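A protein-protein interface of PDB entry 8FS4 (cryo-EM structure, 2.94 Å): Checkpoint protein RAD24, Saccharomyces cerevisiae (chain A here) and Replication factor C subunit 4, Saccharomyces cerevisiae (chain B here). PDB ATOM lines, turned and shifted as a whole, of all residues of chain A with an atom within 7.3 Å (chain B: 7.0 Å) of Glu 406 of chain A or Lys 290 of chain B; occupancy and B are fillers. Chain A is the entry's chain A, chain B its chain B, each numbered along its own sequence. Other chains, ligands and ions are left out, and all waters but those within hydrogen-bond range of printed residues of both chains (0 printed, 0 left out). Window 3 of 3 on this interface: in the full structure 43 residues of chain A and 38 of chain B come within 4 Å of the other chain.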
ATOM      1  N   SER A 399     -18.572 -27.791  12.927  1.00  0.00           N
ATOM      2  CA  SER A 399     -19.382 -28.035  11.738  1.00  0.00           C
ATOM      3  C   SER A 399     -20.867 -28.002  12.072  1.00  0.00           C
ATOM      4  O   SER A 399     -21.663 -27.398  11.342  1.00  0.00           O
ATOM      5  CB  SER A 399     -19.004 -29.376  11.112  1.00  0.00           C
ATOM      6  OG  SER A 399     -17.645 -29.387  10.712  1.00  0.00           O
ATOM      7  N   ILE A 400     -21.258 -28.632  13.180  1.00  0.00           N
ATOM      8  CA  ILE A 400     -22.667 -28.666  13.557  1.00  0.00           C
ATOM      9  C   ILE A 400     -23.186 -27.254  13.795  1.00  0.00           C
ATOM     10  O   ILE A 400     -24.235 -26.860  13.268  1.00  0.00           O
ATOM     11  CB  ILE A 400     -22.865 -29.556  14.798  1.00  0.00           C
ATOM     12  CG1 ILE A 400     -22.725 -31.029  14.406  1.00  0.00           C
ATOM     13  CG2 ILE A 400     -24.219 -29.280  15.450  1.00  0.00           C
ATOM     14  CD1 ILE A 400     -22.805 -31.994  15.566  1.00  0.00           C
ATOM     15  N   VAL A 401     -22.463 -26.469  14.596  1.00  0.00           N
ATOM     16  CA  VAL A 401     -22.958 -25.136  14.930  1.00  0.00           C
ATOM     17  C   VAL A 401     -22.916 -24.222  13.713  1.00  0.00           C
ATOM     18  O   VAL A 401     -23.799 -23.374  13.539  1.00  0.00           O
ATOM     19  CB  VAL A 401     -22.177 -24.538  16.113  1.00  0.00           C
ATOM     20  CG1 VAL A 401     -22.796 -23.223  16.531  1.00  0.00           C
ATOM     21  CG2 VAL A 401     -22.180 -25.494  17.290  1.00  0.00           C
ATOM     22  N   ASP A 402     -21.903 -24.360  12.856  1.00  0.00           N
ATOM     23  CA  ASP A 402     -21.858 -23.563  11.637  1.00  0.00           C
ATOM     24  C   ASP A 402     -23.046 -23.874  10.742  1.00  0.00           C
ATOM     25  O   ASP A 402     -23.657 -22.965  10.172  1.00  0.00           O
ATOM     26  CB  ASP A 402     -20.549 -23.819  10.894  1.00  0.00           C
ATOM     27  CG  ASP A 402     -20.579 -23.305   9.471  1.00  0.00           C
ATOM     28  OD1 ASP A 402     -21.041 -24.047   8.579  1.00  0.00           O
ATOM     29  OD2 ASP A 402     -20.138 -22.161   9.242  1.00  0.00           O
ATOM     30  N   CYS A 403     -23.388 -25.157  10.603  1.00  0.00           N
ATOM     31  CA  CYS A 403     -24.552 -25.516   9.803  1.00  0.00           C
ATOM     32  C   CYS A 403     -25.833 -24.962  10.412  1.00  0.00           C
ATOM     33  O   CYS A 403     -26.721 -24.499   9.689  1.00  0.00           O
ATOM     34  CB  CYS A 403     -24.657 -27.029   9.670  1.00  0.00           C
ATOM     35  SG  CYS A 403     -26.343 -27.545   9.362  1.00  0.00           S
ATOM     36  N   LEU A 404     -25.960 -25.027  11.738  1.00  0.00           N
ATOM     37  CA  LEU A 404     -27.151 -24.479  12.381  1.00  0.00           C
ATOM     38  C   LEU A 404     -27.265 -22.979  12.135  1.00  0.00           C
ATOM     39  O   LEU A 404     -28.352 -22.468  11.844  1.00  0.00           O
ATOM     40  CB  LEU A 404     -27.127 -24.778  13.879  1.00  0.00           C
ATOM     41  CG  LEU A 404     -28.179 -25.765  14.388  1.00  0.00           C
ATOM     42  CD1 LEU A 404     -28.101 -27.087  13.645  1.00  0.00           C
ATOM     43  CD2 LEU A 404     -28.005 -25.982  15.875  1.00  0.00           C
ATOM     44  N   SER A 405     -26.148 -22.256  12.237  1.00  0.00           N
ATOM     45  CA  SER A 405     -26.172 -20.825  11.955  1.00  0.00           C
ATOM     46  C   SER A 405     -26.536 -20.559  10.501  1.00  0.00           C
ATOM     47  O   SER A 405     -27.304 -19.638  10.206  1.00  0.00           O
ATOM     48  CB  SER A 405     -24.818 -20.200  12.287  1.00  0.00           C
ATOM     49  OG  SER A 405     -23.834 -20.596  11.352  1.00  0.00           O
ATOM     50  N   GLU A 406     -25.989 -21.349   9.575  1.00  0.00           N
ATOM     51  CA  GLU A 406     -26.299 -21.149   8.163  1.00  0.00           C
ATOM     52  C   GLU A 406     -27.776 -21.384   7.888  1.00  0.00           C
ATOM     53  O   GLU A 406     -28.406 -20.626   7.142  1.00  0.00           O
ATOM     54  CB  GLU A 406     -25.445 -22.072   7.297  1.00  0.00           C
ATOM     55  CG  GLU A 406     -25.125 -21.499   5.927  1.00  0.00           C
ATOM     56  CD  GLU A 406     -23.897 -22.127   5.297  1.00  0.00           C
ATOM     57  OE1 GLU A 406     -23.325 -23.059   5.901  1.00  0.00           O
ATOM     58  OE2 GLU A 406     -23.502 -21.685   4.197  1.00  0.00           O
ATOM     59  N   CYS A 407     -28.347 -22.436   8.475  1.00  0.00           N
ATOM     60  CA  CYS A 407     -29.762 -22.720   8.277  1.00  0.00           C
ATOM     61  C   CYS A 407     -30.654 -21.735   9.017  1.00  0.00           C
ATOM     62  O   CYS A 407     -31.836 -21.618   8.680  1.00  0.00           O
ATOM     63  CB  CYS A 407     -30.080 -24.148   8.724  1.00  0.00           C
ATOM     64  SG  CYS A 407     -30.692 -24.281  10.413  1.00  0.00           S
ATOM     65  N   ASP A 408     -30.125 -21.035  10.021  1.00  0.00           N
ATOM     66  CA  ASP A 408     -30.909 -20.000  10.687  1.00  0.00           C
ATOM     67  C   ASP A 408     -31.157 -18.790   9.799  1.00  0.00           C
ATOM     68  O   ASP A 408     -32.096 -18.033  10.059  1.00  0.00           O
ATOM     69  CB  ASP A 408     -30.216 -19.545  11.966  1.00  0.00           C
ATOM     70  CG  ASP A 408     -31.072 -18.602  12.777  1.00  0.00           C
ATOM     71  OD1 ASP A 408     -32.249 -18.933  13.023  1.00  0.00           O
ATOM     72  OD2 ASP A 408     -30.573 -17.524  13.158  1.00  0.00           O
ATOM     73  N   ASN A 409     -30.336 -18.581   8.769  1.00  0.00           N
ATOM     74  CA  ASN A 409     -30.523 -17.476   7.837  1.00  0.00           C
ATOM     75  C   ASN A 409     -31.145 -17.935   6.524  1.00  0.00           C
ATOM     76  O   ASN A 409     -31.115 -17.200   5.532  1.00  0.00           O
ATOM     77  CB  ASN A 409     -29.194 -16.734   7.631  1.00  0.00           C
ATOM     78  CG  ASN A 409     -28.359 -17.257   6.462  1.00  0.00           C
ATOM     79  OD1 ASN A 409     -28.762 -18.138   5.704  1.00  0.00           O
ATOM     80  ND2 ASN A 409     -27.173 -16.681   6.309  1.00  0.00           N
ATOM     81  N   MET A 410     -31.715 -19.138   6.505  1.00  0.00           N
ATOM     82  CA  MET A 410     -32.476 -19.647   5.374  1.00  0.00           C
ATOM     83  C   MET A 410     -33.964 -19.371   5.523  1.00  0.00           C
ATOM     84  O   MET A 410     -34.768 -19.967   4.801  1.00  0.00           O
ATOM     85  CB  MET A 410     -32.249 -21.151   5.219  1.00  0.00           C
ATOM     86  CG  MET A 410     -32.008 -21.623   3.797  1.00  0.00           C
ATOM     87  SD  MET A 410     -30.959 -23.088   3.758  1.00  0.00           S
ATOM     88  CE  MET A 410     -29.353 -22.342   3.553  1.00  0.00           C
ATOM     89  N   ASN A 411     -34.345 -18.503   6.461  1.00  0.00           N
ATOM     90  CA  ASN A 411     -35.743 -18.187   6.731  1.00  0.00           C
ATOM     91  C   ASN A 411     -36.417 -19.404   7.352  1.00  0.00           C
ATOM     92  O   ASN A 411     -35.731 -20.290   7.875  1.00  0.00           O
ATOM     93  CB  ASN A 411     -36.456 -17.727   5.451  1.00  0.00           C
ATOM     94  CG  ASN A 411     -36.477 -16.222   5.312  1.00  0.00           C
ATOM     95  OD1 ASN A 411     -35.661 -15.638   4.599  1.00  0.00           O
ATOM     96  ND2 ASN A 411     -37.423 -15.583   5.989  1.00  0.00           N
ATOM     97  N   GLU A 415     -36.443 -26.487   3.596  1.00  0.00           N
ATOM     98  CA  GLU A 415     -35.127 -27.063   3.338  1.00  0.00           C
ATOM     99  C   GLU A 415     -34.168 -26.832   4.497  1.00  0.00           C
ATOM    100  O   GLU A 415     -33.239 -27.623   4.694  1.00  0.00           O
ATOM    101  CB  GLU A 415     -34.536 -26.481   2.055  1.00  0.00           C
ATOM    102  CG  GLU A 415     -35.252 -26.912   0.794  1.00  0.00           C
ATOM    103  CD  GLU A 415     -36.335 -25.941   0.375  1.00  0.00           C
ATOM    104  OE1 GLU A 415     -36.874 -25.238   1.254  1.00  0.00           O
ATOM    105  OE2 GLU A 415     -36.648 -25.883  -0.832  1.00  0.00           O
ATOM    106  N   SER A 416     -34.370 -25.765   5.270  1.00  0.00           N
ATOM    107  CA  SER A 416     -33.421 -25.432   6.328  1.00  0.00           C
ATOM    108  C   SER A 416     -33.344 -26.541   7.370  1.00  0.00           C
ATOM    109  O   SER A 416     -32.252 -26.999   7.725  1.00  0.00           O
ATOM    110  CB  SER A 416     -33.814 -24.109   6.979  1.00  0.00           C
ATOM    111  OG  SER A 416     -34.934 -24.275   7.827  1.00  0.00           O
ATOM    112  N   GLU A 418     -34.436 -29.675   7.084  1.00  0.00           N
ATOM    113  CA  GLU A 418     -34.008 -30.919   6.459  1.00  0.00           C
ATOM    114  C   GLU A 418     -32.502 -30.947   6.257  1.00  0.00           C
ATOM    115  O   GLU A 418     -31.897 -32.026   6.245  1.00  0.00           O
ATOM    116  CB  GLU A 418     -34.727 -31.105   5.126  1.00  0.00           C
ATOM    117  CG  GLU A 418     -36.229 -31.299   5.272  1.00  0.00           C
ATOM    118  CD  GLU A 418     -36.713 -32.649   4.774  1.00  0.00           C
ATOM    119  OE1 GLU A 418     -35.873 -33.538   4.517  1.00  0.00           O
ATOM    120  OE2 GLU A 418     -37.942 -32.825   4.643  1.00  0.00           O
ATOM    121  N   TYR A 419     -31.881 -29.782   6.084  1.00  0.00           N
ATOM    122  CA  TYR A 419     -30.429 -29.728   5.988  1.00  0.00           C
ATOM    123  C   TYR A 419     -29.781 -29.815   7.362  1.00  0.00           C
ATOM    124  O   TYR A 419     -28.812 -30.559   7.549  1.00  0.00           O
ATOM    125  CB  TYR A 419     -30.007 -28.444   5.278  1.00  0.00           C
ATOM    126  CG  TYR A 419     -28.543 -28.107   5.423  1.00  0.00           C
ATOM    127  CD1 TYR A 419     -27.565 -28.943   4.917  1.00  0.00           C
ATOM    128  CD2 TYR A 419     -28.139 -26.947   6.066  1.00  0.00           C
ATOM    129  CE1 TYR A 419     -26.230 -28.629   5.044  1.00  0.00           C
ATOM    130  CE2 TYR A 419     -26.802 -26.632   6.197  1.00  0.00           C
ATOM    131  CZ  TYR A 419     -25.854 -27.484   5.685  1.00  0.00           C
ATOM    132  OH  TYR A 419     -24.513 -27.196   5.798  1.00  0.00           O
ATOM    133  N   THR B 274     -35.009 -34.748  -4.209  1.00  0.00           N
ATOM    134  CA  THR B 274     -33.823 -34.978  -3.394  1.00  0.00           C
ATOM    135  C   THR B 274     -34.178 -35.711  -2.109  1.00  0.00           C
ATOM    136  O   THR B 274     -33.436 -36.595  -1.667  1.00  0.00           O
ATOM    137  CB  THR B 274     -33.138 -33.648  -3.084  1.00  0.00           C
ATOM    138  OG1 THR B 274     -32.455 -33.179  -4.251  1.00  0.00           O
ATOM    139  CG2 THR B 274     -32.139 -33.806  -1.953  1.00  0.00           C
ATOM    140  N   VAL B 284     -23.956 -35.990   0.451  1.00  0.00           N
ATOM    141  CA  VAL B 284     -24.323 -35.396  -0.830  1.00  0.00           C
ATOM    142  C   VAL B 284     -25.776 -34.943  -0.804  1.00  0.00           C
ATOM    143  O   VAL B 284     -26.111 -33.856  -1.287  1.00  0.00           O
ATOM    144  CB  VAL B 284     -24.057 -36.393  -1.972  1.00  0.00           C
ATOM    145  CG1 VAL B 284     -24.711 -35.927  -3.264  1.00  0.00           C
ATOM    146  CG2 VAL B 284     -22.567 -36.577  -2.168  1.00  0.00           C
ATOM    147  N   ARG B 285     -26.664 -35.769  -0.247  1.00  0.00           N
ATOM    148  CA  ARG B 285     -28.076 -35.409  -0.225  1.00  0.00           C
ATOM    149  C   ARG B 285     -28.309 -34.138   0.577  1.00  0.00           C
ATOM    150  O   ARG B 285     -29.062 -33.257   0.149  1.00  0.00           O
ATOM    151  CB  ARG B 285     -28.907 -36.557   0.345  1.00  0.00           C
ATOM    152  CG  ARG B 285     -30.405 -36.278   0.373  1.00  0.00           C
ATOM    153  CD  ARG B 285     -31.158 -37.324   1.171  1.00  0.00           C
ATOM    154  NE  ARG B 285     -30.651 -38.667   0.923  1.00  0.00           N
ATOM    155  CZ  ARG B 285     -31.027 -39.434  -0.090  1.00  0.00           C
ATOM    156  NH1 ARG B 285     -31.926 -39.028  -0.969  1.00  0.00           N
ATOM    157  NH2 ARG B 285     -30.485 -40.640  -0.226  1.00  0.00           N
ATOM    158  N   LEU B 286     -27.678 -34.019   1.745  1.00  0.00           N
ATOM    159  CA  LEU B 286     -27.896 -32.827   2.555  1.00  0.00           C
ATOM    160  C   LEU B 286     -27.252 -31.596   1.927  1.00  0.00           C
ATOM    161  O   LEU B 286     -27.803 -30.492   2.028  1.00  0.00           O
ATOM    162  CB  LEU B 286     -27.394 -33.057   3.982  1.00  0.00           C
ATOM    163  CG  LEU B 286     -25.895 -32.998   4.258  1.00  0.00           C
ATOM    164  CD1 LEU B 286     -25.522 -31.652   4.785  1.00  0.00           C
ATOM    165  CD2 LEU B 286     -25.508 -34.062   5.258  1.00  0.00           C
ATOM    166  N   GLU B 287     -26.113 -31.754   1.249  1.00  0.00           N
ATOM    167  CA  GLU B 287     -25.548 -30.620   0.525  1.00  0.00           C
ATOM    168  C   GLU B 287     -26.481 -30.158  -0.590  1.00  0.00           C
ATOM    169  O   GLU B 287     -26.677 -28.951  -0.786  1.00  0.00           O
ATOM    170  CB  GLU B 287     -24.177 -30.984  -0.039  1.00  0.00           C
ATOM    171  CG  GLU B 287     -23.108 -31.177   1.019  1.00  0.00           C
ATOM    172  CD  GLU B 287     -22.745 -29.886   1.727  1.00  0.00           C
ATOM    173  OE1 GLU B 287     -22.922 -28.805   1.126  1.00  0.00           O
ATOM    174  OE2 GLU B 287     -22.285 -29.951   2.886  1.00  0.00           O
ATOM    175  N   MET B 288     -27.065 -31.101  -1.334  1.00  0.00           N
ATOM    176  CA  MET B 288     -28.014 -30.725  -2.378  1.00  0.00           C
ATOM    177  C   MET B 288     -29.246 -30.062  -1.783  1.00  0.00           C
ATOM    178  O   MET B 288     -29.796 -29.122  -2.366  1.00  0.00           O
ATOM    179  CB  MET B 288     -28.414 -31.946  -3.204  1.00  0.00           C
ATOM    180  CG  MET B 288     -27.254 -32.605  -3.924  1.00  0.00           C
ATOM    181  SD  MET B 288     -27.662 -34.077  -4.890  1.00  0.00           S
ATOM    182  CE  MET B 288     -29.431 -34.208  -4.670  1.00  0.00           C
ATOM    183  N   ILE B 289     -29.701 -30.541  -0.625  1.00  0.00           N
ATOM    184  CA  ILE B 289     -30.826 -29.898   0.044  1.00  0.00           C
ATOM    185  C   ILE B 289     -30.478 -28.457   0.390  1.00  0.00           C
ATOM    186  O   ILE B 289     -31.300 -27.551   0.232  1.00  0.00           O
ATOM    187  CB  ILE B 289     -31.241 -30.700   1.291  1.00  0.00           C
ATOM    188  CG1 ILE B 289     -32.033 -31.938   0.867  1.00  0.00           C
ATOM    189  CG2 ILE B 289     -32.059 -29.833   2.249  1.00  0.00           C
ATOM    190  CD1 ILE B 289     -32.502 -32.805   2.009  1.00  0.00           C
ATOM    191  N   LYS B 290     -29.259 -28.224   0.880  1.00  0.00           N
ATOM    192  CA  LYS B 290     -28.852 -26.861   1.212  1.00  0.00           C
ATOM    193  C   LYS B 290     -28.820 -25.974  -0.027  1.00  0.00           C
ATOM    194  O   LYS B 290     -29.284 -24.827   0.008  1.00  0.00           O
ATOM    195  CB  LYS B 290     -27.485 -26.875   1.891  1.00  0.00           C
ATOM    196  CG  LYS B 290     -26.937 -25.498   2.232  1.00  0.00           C
ATOM    197  CD  LYS B 290     -25.500 -25.584   2.704  1.00  0.00           C
ATOM    198  CE  LYS B 290     -24.810 -24.237   2.650  1.00  0.00           C
ATOM    199  NZ  LYS B 290     -23.382 -24.343   3.054  1.00  0.00           N
ATOM    200  N   GLU B 291     -28.258 -26.476  -1.128  1.00  0.00           N
ATOM    201  CA  GLU B 291     -28.210 -25.670  -2.346  1.00  0.00           C
ATOM    202  C   GLU B 291     -29.611 -25.363  -2.856  1.00  0.00           C
ATOM    203  O   GLU B 291     -29.898 -24.237  -3.283  1.00  0.00           O
ATOM    204  CB  GLU B 291     -27.394 -26.381  -3.424  1.00  0.00           C
ATOM    205  CG  GLU B 291     -25.959 -26.694  -3.025  1.00  0.00           C
ATOM    206  CD  GLU B 291     -25.251 -25.516  -2.382  1.00  0.00           C
ATOM    207  OE1 GLU B 291     -25.386 -24.386  -2.894  1.00  0.00           O
ATOM    208  OE2 GLU B 291     -24.558 -25.721  -1.363  1.00  0.00           O
ATOM    209  N   ILE B 292     -30.505 -26.351  -2.811  1.00  0.00           N
ATOM    210  CA  ILE B 292     -31.877 -26.135  -3.251  1.00  0.00           C
ATOM    211  C   ILE B 292     -32.574 -25.131  -2.343  1.00  0.00           C
ATOM    212  O   ILE B 292     -33.374 -24.314  -2.806  1.00  0.00           O
ATOM    213  CB  ILE B 292     -32.627 -27.478  -3.308  1.00  0.00           C
ATOM    214  CG1 ILE B 292     -32.135 -28.292  -4.506  1.00  0.00           C
ATOM    215  CG2 ILE B 292     -34.129 -27.259  -3.397  1.00  0.00           C
ATOM    216  CD1 ILE B 292     -32.465 -29.757  -4.427  1.00  0.00           C
ATOM    217  N   GLY B 293     -32.291 -25.174  -1.042  1.00  0.00           N
ATOM    218  CA  GLY B 293     -32.879 -24.201  -0.137  1.00  0.00           C
ATOM    219  C   GLY B 293     -32.397 -22.790  -0.413  1.00  0.00           C
ATOM    220  O   GLY B 293     -33.176 -21.835  -0.363  1.00  0.00           O
ATOM    221  N   LEU B 294     -31.105 -22.638  -0.707  1.00  0.00           N
ATOM    222  CA  LEU B 294     -30.588 -21.321  -1.070  1.00  0.00           C
ATOM    223  C   LEU B 294     -31.230 -20.813  -2.353  1.00  0.00           C
ATOM    224  O   LEU B 294     -31.593 -19.634  -2.453  1.00  0.00           O
ATOM    225  CB  LEU B 294     -29.067 -21.374  -1.215  1.00  0.00           C
ATOM    226  CG  LEU B 294     -28.282 -21.554   0.083  1.00  0.00           C
ATOM    227  CD1 LEU B 294     -26.809 -21.762  -0.201  1.00  0.00           C
ATOM    228  CD2 LEU B 294     -28.473 -20.343   0.980  1.00  0.00           C
ATOM    229  N   THR B 295     -31.377 -21.685  -3.352  1.00  0.00           N
ATOM    230  CA  THR B 295     -32.025 -21.268  -4.591  1.00  0.00           C
ATOM    231  C   THR B 295     -33.484 -20.906  -4.350  1.00  0.00           C
ATOM    232  O   THR B 295     -34.001 -19.959  -4.947  1.00  0.00           O
ATOM    233  CB  THR B 295     -31.917 -22.364  -5.642  1.00  0.00           C
ATOM    234  OG1 THR B 295     -30.560 -22.805  -5.730  1.00  0.00           O
ATOM    235  CG2 THR B 295     -32.367 -21.847  -6.997  1.00  0.00           C
ATOM    236  N   HIS B 296     -34.170 -21.661  -3.493  1.00  0.00           N
ATOM    237  CA  HIS B 296     -35.543 -21.323  -3.142  1.00  0.00           C
ATOM    238  C   HIS B 296     -35.611 -19.953  -2.486  1.00  0.00           C
ATOM    239  O   HIS B 296     -36.515 -19.161  -2.772  1.00  0.00           O
ATOM    240  CB  HIS B 296     -36.111 -22.394  -2.213  1.00  0.00           C
ATOM    241  CG  HIS B 296     -37.603 -22.393  -2.121  1.00  0.00           C
ATOM    242  ND1 HIS B 296     -38.312 -21.371  -1.528  1.00  0.00           N
ATOM    243  CD2 HIS B 296     -38.521 -23.297  -2.532  1.00  0.00           C
ATOM    244  CE1 HIS B 296     -39.603 -21.642  -1.585  1.00  0.00           C
ATOM    245  NE2 HIS B 296     -39.758 -22.806  -2.190  1.00  0.00           N
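OE2 of Glu 406 of chain A is in salt-bridge range of NZ of Lys 290 of chain B (2.9 Å).
O of Glu 406 of chain A sits close to OD1 of Asn 409 of chain A, 2.9 Å away.
Met 410 of chain A touches Leu 294 of chain B (CE to CD2, 3.4 Å).
O of Glu 415 of chain A touches CG2 of Ile 289 of chain B (3.5 Å).
Glu 415 of chain A touches Ile 292 of chain B (OE2 to CG2, 3.8 Å).
CB of Glu 415 of chain A touches CA of Gly 293 of chain B, 3.6 Å away.
His 296 of chain B touches Glu 415 of chain A (CD2 to OE2, 3.6 Å).
CE1 of Tyr 419 of chain A touches CD1 of Leu 286 of chain B (3.1 Å).
CG2 of Ile 289 of chain B touches N of Tyr 419 of chain A, 3.8 Å away.
CZ of Tyr 419 of chain A touches CD of Lys 290 of chain B (3.6 Å).
Leu 404 of chain A touches none of the printed residues of chain B.
Glu 406 of chain A touches one residue of chain B.
Of the printed residues of chain B, Met 410 of chain A touches Leu 294.
Of the printed residues of chain B, Glu 415 of chain A touches Ile 289 (3.5 Å), Ile 292 (3.8 Å), Gly 293 (3.6 Å) and His 296 (3.6 Å).
Of chain A, only Glu 406 and Tyr 419 come within 4 Å of Lys 290 of chain B.
Of the printed residues of chain A, Leu 294 of chain B touches Met 410 (3.4 Å).
Of the printed residues of chain A, His 296 of chain B touches Glu 415 (3.6 Å).
The nearest residue of chain B that does not touch Glu 406 of chain A is Leu 294 of chain B (5.5 Å).
The nearest residue of chain A that does not touch Lys 290 of chain B is Met 410 of chain A (4.2 Å).
The nearest printed residue of chain A that does not touch Leu 286 of chain B is Glu 418 of chain A (5.1 Å).
Of the 17 printed residues of chain A, 4 touch a printed residue of chain B.
Printed residues of chain A that touch a printed residue of chain B: Glu 406, Met 410, Glu 415 and Tyr 419.
Hydrophobic or aromatic side chains of chain A within 4 Å of the printed part of chain B: Met 410 and Tyr 419.
Among the printed residues, 9 pairs touch across the chains.
Among the printed residues, Asp or Glu carboxylates within 4 Å of a Lys or Arg side-chain nitrogen of the other chain: Glu 406 of chain A with Lys 290 of chain B.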
